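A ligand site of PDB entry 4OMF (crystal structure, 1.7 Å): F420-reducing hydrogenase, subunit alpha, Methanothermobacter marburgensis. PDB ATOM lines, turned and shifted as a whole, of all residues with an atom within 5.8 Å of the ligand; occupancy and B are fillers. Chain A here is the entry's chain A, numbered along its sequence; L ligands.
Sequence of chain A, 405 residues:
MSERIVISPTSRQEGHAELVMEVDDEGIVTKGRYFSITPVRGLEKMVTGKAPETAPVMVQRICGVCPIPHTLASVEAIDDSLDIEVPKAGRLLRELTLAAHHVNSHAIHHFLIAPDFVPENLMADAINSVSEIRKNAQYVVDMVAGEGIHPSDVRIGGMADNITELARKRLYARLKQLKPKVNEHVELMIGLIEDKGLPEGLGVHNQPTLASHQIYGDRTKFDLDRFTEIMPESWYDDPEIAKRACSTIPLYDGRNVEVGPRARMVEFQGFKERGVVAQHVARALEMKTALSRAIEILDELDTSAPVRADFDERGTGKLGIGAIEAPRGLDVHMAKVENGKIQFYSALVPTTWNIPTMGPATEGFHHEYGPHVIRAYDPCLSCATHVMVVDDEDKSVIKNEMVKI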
ATOM      1  N   GLU A  14      18.110  19.885  -9.394  1.00  0.00           N
ATOM      2  CA  GLU A  14      16.662  19.978  -9.150  1.00  0.00           C
ATOM      3  C   GLU A  14      16.110  18.621  -8.759  1.00  0.00           C
ATOM      4  O   GLU A  14      16.411  17.625  -9.405  1.00  0.00           O
ATOM      5  CB  GLU A  14      15.923  20.504 -10.373  1.00  0.00           C
ATOM      6  CG  GLU A  14      14.477  20.947 -10.092  1.00  0.00           C
ATOM      7  CD  GLU A  14      13.498  19.789  -9.869  1.00  0.00           C
ATOM      8  OE1 GLU A  14      13.764  18.666 -10.357  1.00  0.00           O
ATOM      9  OE2 GLU A  14      12.478  20.017  -9.177  1.00  0.00           O
ATOM     10  N   CYS A  63       8.132  21.155 -14.356  1.00  0.00           N
ATOM     11  CA  CYS A  63       9.364  21.742 -13.841  1.00  0.00           C
ATOM     12  C   CYS A  63       9.429  23.250 -13.968  1.00  0.00           C
ATOM     13  O   CYS A  63       9.197  23.803 -15.065  1.00  0.00           O
ATOM     14  CB  CYS A  63      10.572  21.165 -14.583  1.00  0.00           C
ATOM     15  SG  CYS A  63      12.104  21.786 -13.839  1.00  0.00           S
ATOM     16  N   GLY A  64       9.780  23.919 -12.857  1.00  0.00           N
ATOM     17  CA  GLY A  64       9.842  25.379 -12.841  1.00  0.00           C
ATOM     18  C   GLY A  64      11.230  25.935 -13.120  1.00  0.00           C
ATOM     19  O   GLY A  64      11.431  27.159 -13.143  1.00  0.00           O
ATOM     20  N   VAL A  65      12.196  25.037 -13.318  1.00  0.00           N
ATOM     21  CA  VAL A  65      13.525  25.405 -13.818  1.00  0.00           C
ATOM     22  C   VAL A  65      13.463  25.483 -15.329  1.00  0.00           C
ATOM     23  O   VAL A  65      13.964  26.455 -15.927  1.00  0.00           O
ATOM     24  CB  VAL A  65      14.608  24.388 -13.372  1.00  0.00           C
ATOM     25  CG1 VAL A  65      15.950  24.715 -14.039  1.00  0.00           C
ATOM     26  CG2 VAL A  65      14.754  24.401 -11.854  1.00  0.00           C
ATOM     27  N   CYS A  66      12.837  24.489 -15.957  1.00  0.00           N
ATOM     28  CA  CYS A  66      12.761  24.442 -17.421  1.00  0.00           C
ATOM     29  C   CYS A  66      11.362  24.337 -18.014  1.00  0.00           C
ATOM     30  O   CYS A  66      11.149  23.547 -18.942  1.00  0.00           O
ATOM     31  CB  CYS A  66      13.565  23.256 -17.946  1.00  0.00           C
ATOM     32  SG  CYS A  66      12.776  21.714 -17.381  1.00  0.00           S
ATOM     33  N   PRO A  69      10.758  24.542 -22.380  1.00  0.00           N
ATOM     34  CA  PRO A  69      10.716  23.483 -23.405  1.00  0.00           C
ATOM     35  C   PRO A  69       9.547  22.492 -23.300  1.00  0.00           C
ATOM     36  O   PRO A  69       9.157  21.958 -24.341  1.00  0.00           O
ATOM     37  CB  PRO A  69      12.060  22.744 -23.199  1.00  0.00           C
ATOM     38  CG  PRO A  69      12.512  23.110 -21.794  1.00  0.00           C
ATOM     39  CD  PRO A  69      12.055  24.566 -21.685  1.00  0.00           C
ATOM     40  N   HIS A  70       9.009  22.252 -22.099  1.00  0.00           N
ATOM     41  CA  HIS A  70       7.808  21.440 -22.017  1.00  0.00           C
ATOM     42  C   HIS A  70       6.622  22.096 -22.693  1.00  0.00           C
ATOM     43  O   HIS A  70       5.855  21.413 -23.367  1.00  0.00           O
ATOM     44  CB  HIS A  70       7.474  21.127 -20.564  1.00  0.00           C
ATOM     45  CG  HIS A  70       8.471  20.228 -19.909  1.00  0.00           C
ATOM     46  ND1 HIS A  70       8.834  19.008 -20.438  1.00  0.00           N
ATOM     47  CD2 HIS A  70       9.193  20.375 -18.771  1.00  0.00           C
ATOM     48  CE1 HIS A  70       9.737  18.443 -19.647  1.00  0.00           C
ATOM     49  NE2 HIS A  70       9.964  19.250 -18.630  1.00  0.00           N
ATOM     50  N   HIS A 101      15.846  31.066 -23.025  1.00  0.00           N
ATOM     51  CA  HIS A 101      15.686  30.144 -21.907  1.00  0.00           C
ATOM     52  C   HIS A 101      16.961  29.365 -21.651  1.00  0.00           C
ATOM     53  O   HIS A 101      17.338  29.161 -20.491  1.00  0.00           O
ATOM     54  CB  HIS A 101      14.547  29.175 -22.173  1.00  0.00           C
ATOM     55  CG  HIS A 101      14.350  28.181 -21.062  1.00  0.00           C
ATOM     56  ND1 HIS A 101      13.995  28.565 -19.796  1.00  0.00           N
ATOM     57  CD2 HIS A 101      14.491  26.832 -21.028  1.00  0.00           C
ATOM     58  CE1 HIS A 101      13.900  27.500 -19.017  1.00  0.00           C
ATOM     59  NE2 HIS A 101      14.175  26.432 -19.749  1.00  0.00           N
ATOM     60  N   SER A 105      18.797  29.026 -18.055  1.00  0.00           N
ATOM     61  CA  SER A 105      18.936  27.706 -17.412  1.00  0.00           C
ATOM     62  C   SER A 105      20.394  27.307 -17.154  1.00  0.00           C
ATOM     63  O   SER A 105      20.717  26.761 -16.095  1.00  0.00           O
ATOM     64  CB  SER A 105      18.244  26.627 -18.247  1.00  0.00           C
ATOM     65  OG  SER A 105      18.353  25.334 -17.627  1.00  0.00           O
ATOM     66  N   ALA A 326      15.664  20.865 -24.936  1.00  0.00           N
ATOM     67  CA  ALA A 326      15.667  21.542 -23.637  1.00  0.00           C
ATOM     68  C   ALA A 326      17.095  21.840 -23.226  1.00  0.00           C
ATOM     69  O   ALA A 326      18.048  21.238 -23.745  1.00  0.00           O
ATOM     70  CB  ALA A 326      14.969  20.661 -22.590  1.00  0.00           C
ATOM     71  N   PRO A 327      17.270  22.763 -22.278  1.00  0.00           N
ATOM     72  CA  PRO A 327      18.646  22.994 -21.834  1.00  0.00           C
ATOM     73  C   PRO A 327      19.375  21.715 -21.384  1.00  0.00           C
ATOM     74  O   PRO A 327      20.586  21.604 -21.595  1.00  0.00           O
ATOM     75  CB  PRO A 327      18.476  23.978 -20.662  1.00  0.00           C
ATOM     76  CG  PRO A 327      17.198  24.725 -20.986  1.00  0.00           C
ATOM     77  CD  PRO A 327      16.299  23.673 -21.640  1.00  0.00           C
ATOM     78  N   ARG A 328      18.667  20.751 -20.803  1.00  0.00           N
ATOM     79  CA  ARG A 328      19.306  19.522 -20.339  1.00  0.00           C
ATOM     80  C   ARG A 328      19.330  18.396 -21.387  1.00  0.00           C
ATOM     81  O   ARG A 328      19.907  17.334 -21.147  1.00  0.00           O
ATOM     82  CB  ARG A 328      18.616  19.038 -19.048  1.00  0.00           C
ATOM     83  CG  ARG A 328      18.905  20.027 -17.910  1.00  0.00           C
ATOM     84  CD  ARG A 328      17.970  20.035 -16.679  1.00  0.00           C
ATOM     85  NE  ARG A 328      18.542  21.062 -15.824  1.00  0.00           N
ATOM     86  CZ  ARG A 328      18.296  22.370 -15.959  1.00  0.00           C
ATOM     87  NH1 ARG A 328      18.931  23.240 -15.172  1.00  0.00           N
ATOM     88  NH2 ARG A 328      17.397  22.797 -16.861  1.00  0.00           N
ATOM     89  N   GLY A 329      18.717  18.616 -22.546  1.00  0.00           N
ATOM     90  CA  GLY A 329      18.728  17.624 -23.604  1.00  0.00           C
ATOM     91  C   GLY A 329      17.401  17.425 -24.298  1.00  0.00           C
ATOM     92  O   GLY A 329      16.399  18.137 -24.059  1.00  0.00           O
ATOM     93  N   ASP A 331      13.897  16.632 -25.340  1.00  0.00           N
ATOM     94  CA  ASP A 331      12.638  16.566 -24.617  1.00  0.00           C
ATOM     95  C   ASP A 331      11.561  16.214 -25.634  1.00  0.00           C
ATOM     96  O   ASP A 331      11.222  17.067 -26.464  1.00  0.00           O
ATOM     97  CB  ASP A 331      12.364  17.927 -23.944  1.00  0.00           C
ATOM     98  CG  ASP A 331      11.093  17.974 -23.079  1.00  0.00           C
ATOM     99  OD1 ASP A 331      10.615  16.910 -22.614  1.00  0.00           O
ATOM    100  OD2 ASP A 331      10.603  19.111 -22.830  1.00  0.00           O
ATOM    101  N   VAL A 349      11.732  12.927 -21.180  1.00  0.00           N
ATOM    102  CA  VAL A 349      12.344  14.200 -20.792  1.00  0.00           C
ATOM    103  C   VAL A 349      13.864  14.000 -20.615  1.00  0.00           C
ATOM    104  O   VAL A 349      14.297  12.884 -20.346  1.00  0.00           O
ATOM    105  CB  VAL A 349      11.648  14.689 -19.494  1.00  0.00           C
ATOM    106  CG1 VAL A 349      12.149  16.043 -19.014  1.00  0.00           C
ATOM    107  CG2 VAL A 349      10.122  14.749 -19.731  1.00  0.00           C
ATOM    108  N   PRO A 350      14.674  15.048 -20.847  1.00  0.00           N
ATOM    109  CA  PRO A 350      16.121  14.792 -20.910  1.00  0.00           C
ATOM    110  C   PRO A 350      16.685  14.020 -19.717  1.00  0.00           C
ATOM    111  O   PRO A 350      17.463  13.084 -19.919  1.00  0.00           O
ATOM    112  CB  PRO A 350      16.757  16.209 -20.961  1.00  0.00           C
ATOM    113  CG  PRO A 350      15.540  17.197 -21.039  1.00  0.00           C
ATOM    114  CD  PRO A 350      14.352  16.378 -21.387  1.00  0.00           C
ATOM    115  N   THR A 351      16.353  14.404 -18.490  1.00  0.00           N
ATOM    116  CA  THR A 351      16.991  13.720 -17.370  1.00  0.00           C
ATOM    117  C   THR A 351      16.465  12.280 -17.303  1.00  0.00           C
ATOM    118  O   THR A 351      17.161  11.387 -16.829  1.00  0.00           O
ATOM    119  CB  THR A 351      16.773  14.482 -16.064  1.00  0.00           C
ATOM    120  OG1 THR A 351      17.398  15.766 -16.187  1.00  0.00           O
ATOM    121  CG2 THR A 351      17.446  13.744 -14.879  1.00  0.00           C
ATOM    122  N   THR A 352      15.245  12.047 -17.812  1.00  0.00           N
ATOM    123  CA  THR A 352      14.755  10.662 -17.928  1.00  0.00           C
ATOM    124  C   THR A 352      15.748   9.844 -18.762  1.00  0.00           C
ATOM    125  O   THR A 352      16.103   8.722 -18.395  1.00  0.00           O
ATOM    126  CB  THR A 352      13.378  10.576 -18.602  1.00  0.00           C
ATOM    127  OG1 THR A 352      12.477  11.580 -18.097  1.00  0.00           O
ATOM    128  CG2 THR A 352      12.765   9.164 -18.399  1.00  0.00           C
ATOM    129  N   ASP A 378      23.590  18.128 -15.045  1.00  0.00           N
ATOM    130  CA  ASP A 378      22.576  19.140 -14.696  1.00  0.00           C
ATOM    131  C   ASP A 378      21.198  18.475 -14.499  1.00  0.00           C
ATOM    132  O   ASP A 378      20.205  18.866 -15.131  1.00  0.00           O
ATOM    133  CB  ASP A 378      22.557  20.211 -15.800  1.00  0.00           C
ATOM    134  CG  ASP A 378      21.667  21.417 -15.509  1.00  0.00           C
ATOM    135  OD1 ASP A 378      21.148  21.610 -14.397  1.00  0.00           O
ATOM    136  OD2 ASP A 378      21.497  22.189 -16.458  1.00  0.00           O
ATOM    137  N   PRO A 379      21.134  17.436 -13.651  1.00  0.00           N
ATOM    138  CA  PRO A 379      19.897  16.643 -13.631  1.00  0.00           C
ATOM    139  C   PRO A 379      18.710  17.388 -13.030  1.00  0.00           C
ATOM    140  O   PRO A 379      18.850  18.237 -12.118  1.00  0.00           O
ATOM    141  CB  PRO A 379      20.279  15.427 -12.776  1.00  0.00           C
ATOM    142  CG  PRO A 379      21.367  15.946 -11.840  1.00  0.00           C
ATOM    143  CD  PRO A 379      22.150  16.919 -12.729  1.00  0.00           C
ATOM    144  N   CYS A 380      17.546  17.048 -13.549  1.00  0.00           N
ATOM    145  CA  CYS A 380      16.302  17.623 -13.098  1.00  0.00           C
ATOM    146  C   CYS A 380      15.320  16.490 -12.847  1.00  0.00           C
ATOM    147  O   CYS A 380      14.887  15.819 -13.791  1.00  0.00           O
ATOM    148  CB  CYS A 380      15.772  18.585 -14.143  1.00  0.00           C
ATOM    149  SG  CYS A 380      14.408  19.441 -13.414  1.00  0.00           S
ATOM    150  N   SER A 382      12.299  16.422 -11.082  1.00  0.00           N
ATOM    151  CA  SER A 382      10.872  16.661 -11.348  1.00  0.00           C
ATOM    152  C   SER A 382      10.628  16.468 -12.848  1.00  0.00           C
ATOM    153  O   SER A 382       9.661  15.824 -13.240  1.00  0.00           O
ATOM    154  CB  SER A 382      10.426  18.048 -10.893  1.00  0.00           C
ATOM    155  OG  SER A 382      10.589  18.180  -9.502  1.00  0.00           O
ATOM    156  N   CYS A 383      11.537  16.967 -13.672  1.00  0.00           N
ATOM    157  CA  CYS A 383      11.545  16.643 -15.104  1.00  0.00           C
ATOM    158  C   CYS A 383      11.596  15.170 -15.426  1.00  0.00           C
ATOM    159  O   CYS A 383      10.804  14.673 -16.233  1.00  0.00           O
ATOM    160  CB  CYS A 383      12.734  17.300 -15.768  1.00  0.00           C
ATOM    161  SG  CYS A 383      12.281  18.830 -16.476  1.00  0.00           S
ATOM    162  N   ALA A 384      12.566  14.461 -14.855  1.00  0.00           N
ATOM    163  CA  ALA A 384      12.736  13.045 -15.126  1.00  0.00           C
ATOM    164  C   ALA A 384      11.483  12.205 -14.844  1.00  0.00           C
ATOM    165  O   ALA A 384      11.228  11.206 -15.529  1.00  0.00           O
ATOM    166  CB  ALA A 384      13.922  12.483 -14.316  1.00  0.00           C
HETATM  167 FE1  LIG L   1      13.987  19.766 -17.892  1.00  0.00          FE
HETATM  168 NI1  LIG L   1      13.577  20.694 -15.321  1.00  0.00          NI
HETATM  169  C1  LIG L   1      15.308  20.678 -18.789  1.00  0.00           C
HETATM  170  N1  LIG L   1      16.157  21.255 -19.379  1.00  0.00           N
HETATM  171  C2  LIG L   1      15.020  18.250 -17.737  1.00  0.00           C
HETATM  172  N2  LIG L   1      15.622  17.277 -17.612  1.00  0.00           N
HETATM  173  C3  LIG L   1      13.163  19.401 -19.532  1.00  0.00           C
HETATM  174  O1  LIG L   1      12.629  19.184 -20.548  1.00  0.00           O
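N of Thr 351 sits at hydrogen-bond distance from N2 of the ligand, 3.1 Å away.
The side-chain sulfur of Cys 66 binds an iron atom (FE1) of the ligand, 2.3 Å away.
The backbone NH of Arg 328 lies within hydrogen-bond range of a nitrogen (N1) of the ligand (2.9 Å).
The side-chain sulfur (SG) of Cys 63 is bound to a nickel atom (NI1) of the ligand (2.4 Å).
An oxygen (O1) of the ligand lies close to a ring nitrogen (NE2) of His 70 (3.3 Å).
SG of Cys 380 binds NI1 of the ligand, at 2.4 Å.
N2 of the ligand lies within hydrogen-bond range of OG1 of Thr 351, at 2.7 Å.
An iron atom (FE1) of the ligand is bound by the side-chain sulfur of Cys 383, 2.4 Å away.
The guanidinium group (NH2) of Arg 328 is in hydrogen-bond range of a nitrogen (N1) of the ligand, 3.2 Å away.
NH2 of Arg 328 lies within hydrogen-bond range of OG of Ser 105 (2.8 Å).
The side-chain carboxylate (OE1) of Glu 14 lies close to the side-chain sulfur (SG) of Cys 380, 3.2 Å away.
NH1 of Arg 328 is in salt-bridge range of OD1 of Asp 378.
A ring nitrogen (ND1) of His 70 lies within hydrogen-bond range of the side-chain carboxylate of Asp 331, 3.0 Å away.
The side-chain sulfur of Cys 63 lies close to the backbone NH of Val 65 (3.3 Å).
The backbone carbonyl oxygen (O) of Val 349 lies close to the side-chain hydroxyl (OG1) of Thr 352.
NE2 of His 70 sits close to SG of Cys 383, at 3.2 Å.
The backbone NH (N) of Cys 380 is in hydrogen-bond range of the side-chain hydroxyl (OG1) of Thr 351.
N1 of the ligand sits close to N of Pro 327 (3.5 Å).
The side-chain carboxylate (OD2) of Asp 331 lies close to an oxygen (O1) of the ligand, 3.1 Å away.
Ala 326 touches the ligand (CB to O1, 3.4 Å).
Val 349 touches the ligand.
CD of Pro 350 touches O1 of the ligand (3.4 Å).
Of the 24 residues printed, 12 come within 4 Å of the ligand.
The nearest printed residue that does not touch the ligand is Pro 69 (4.1 Å).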
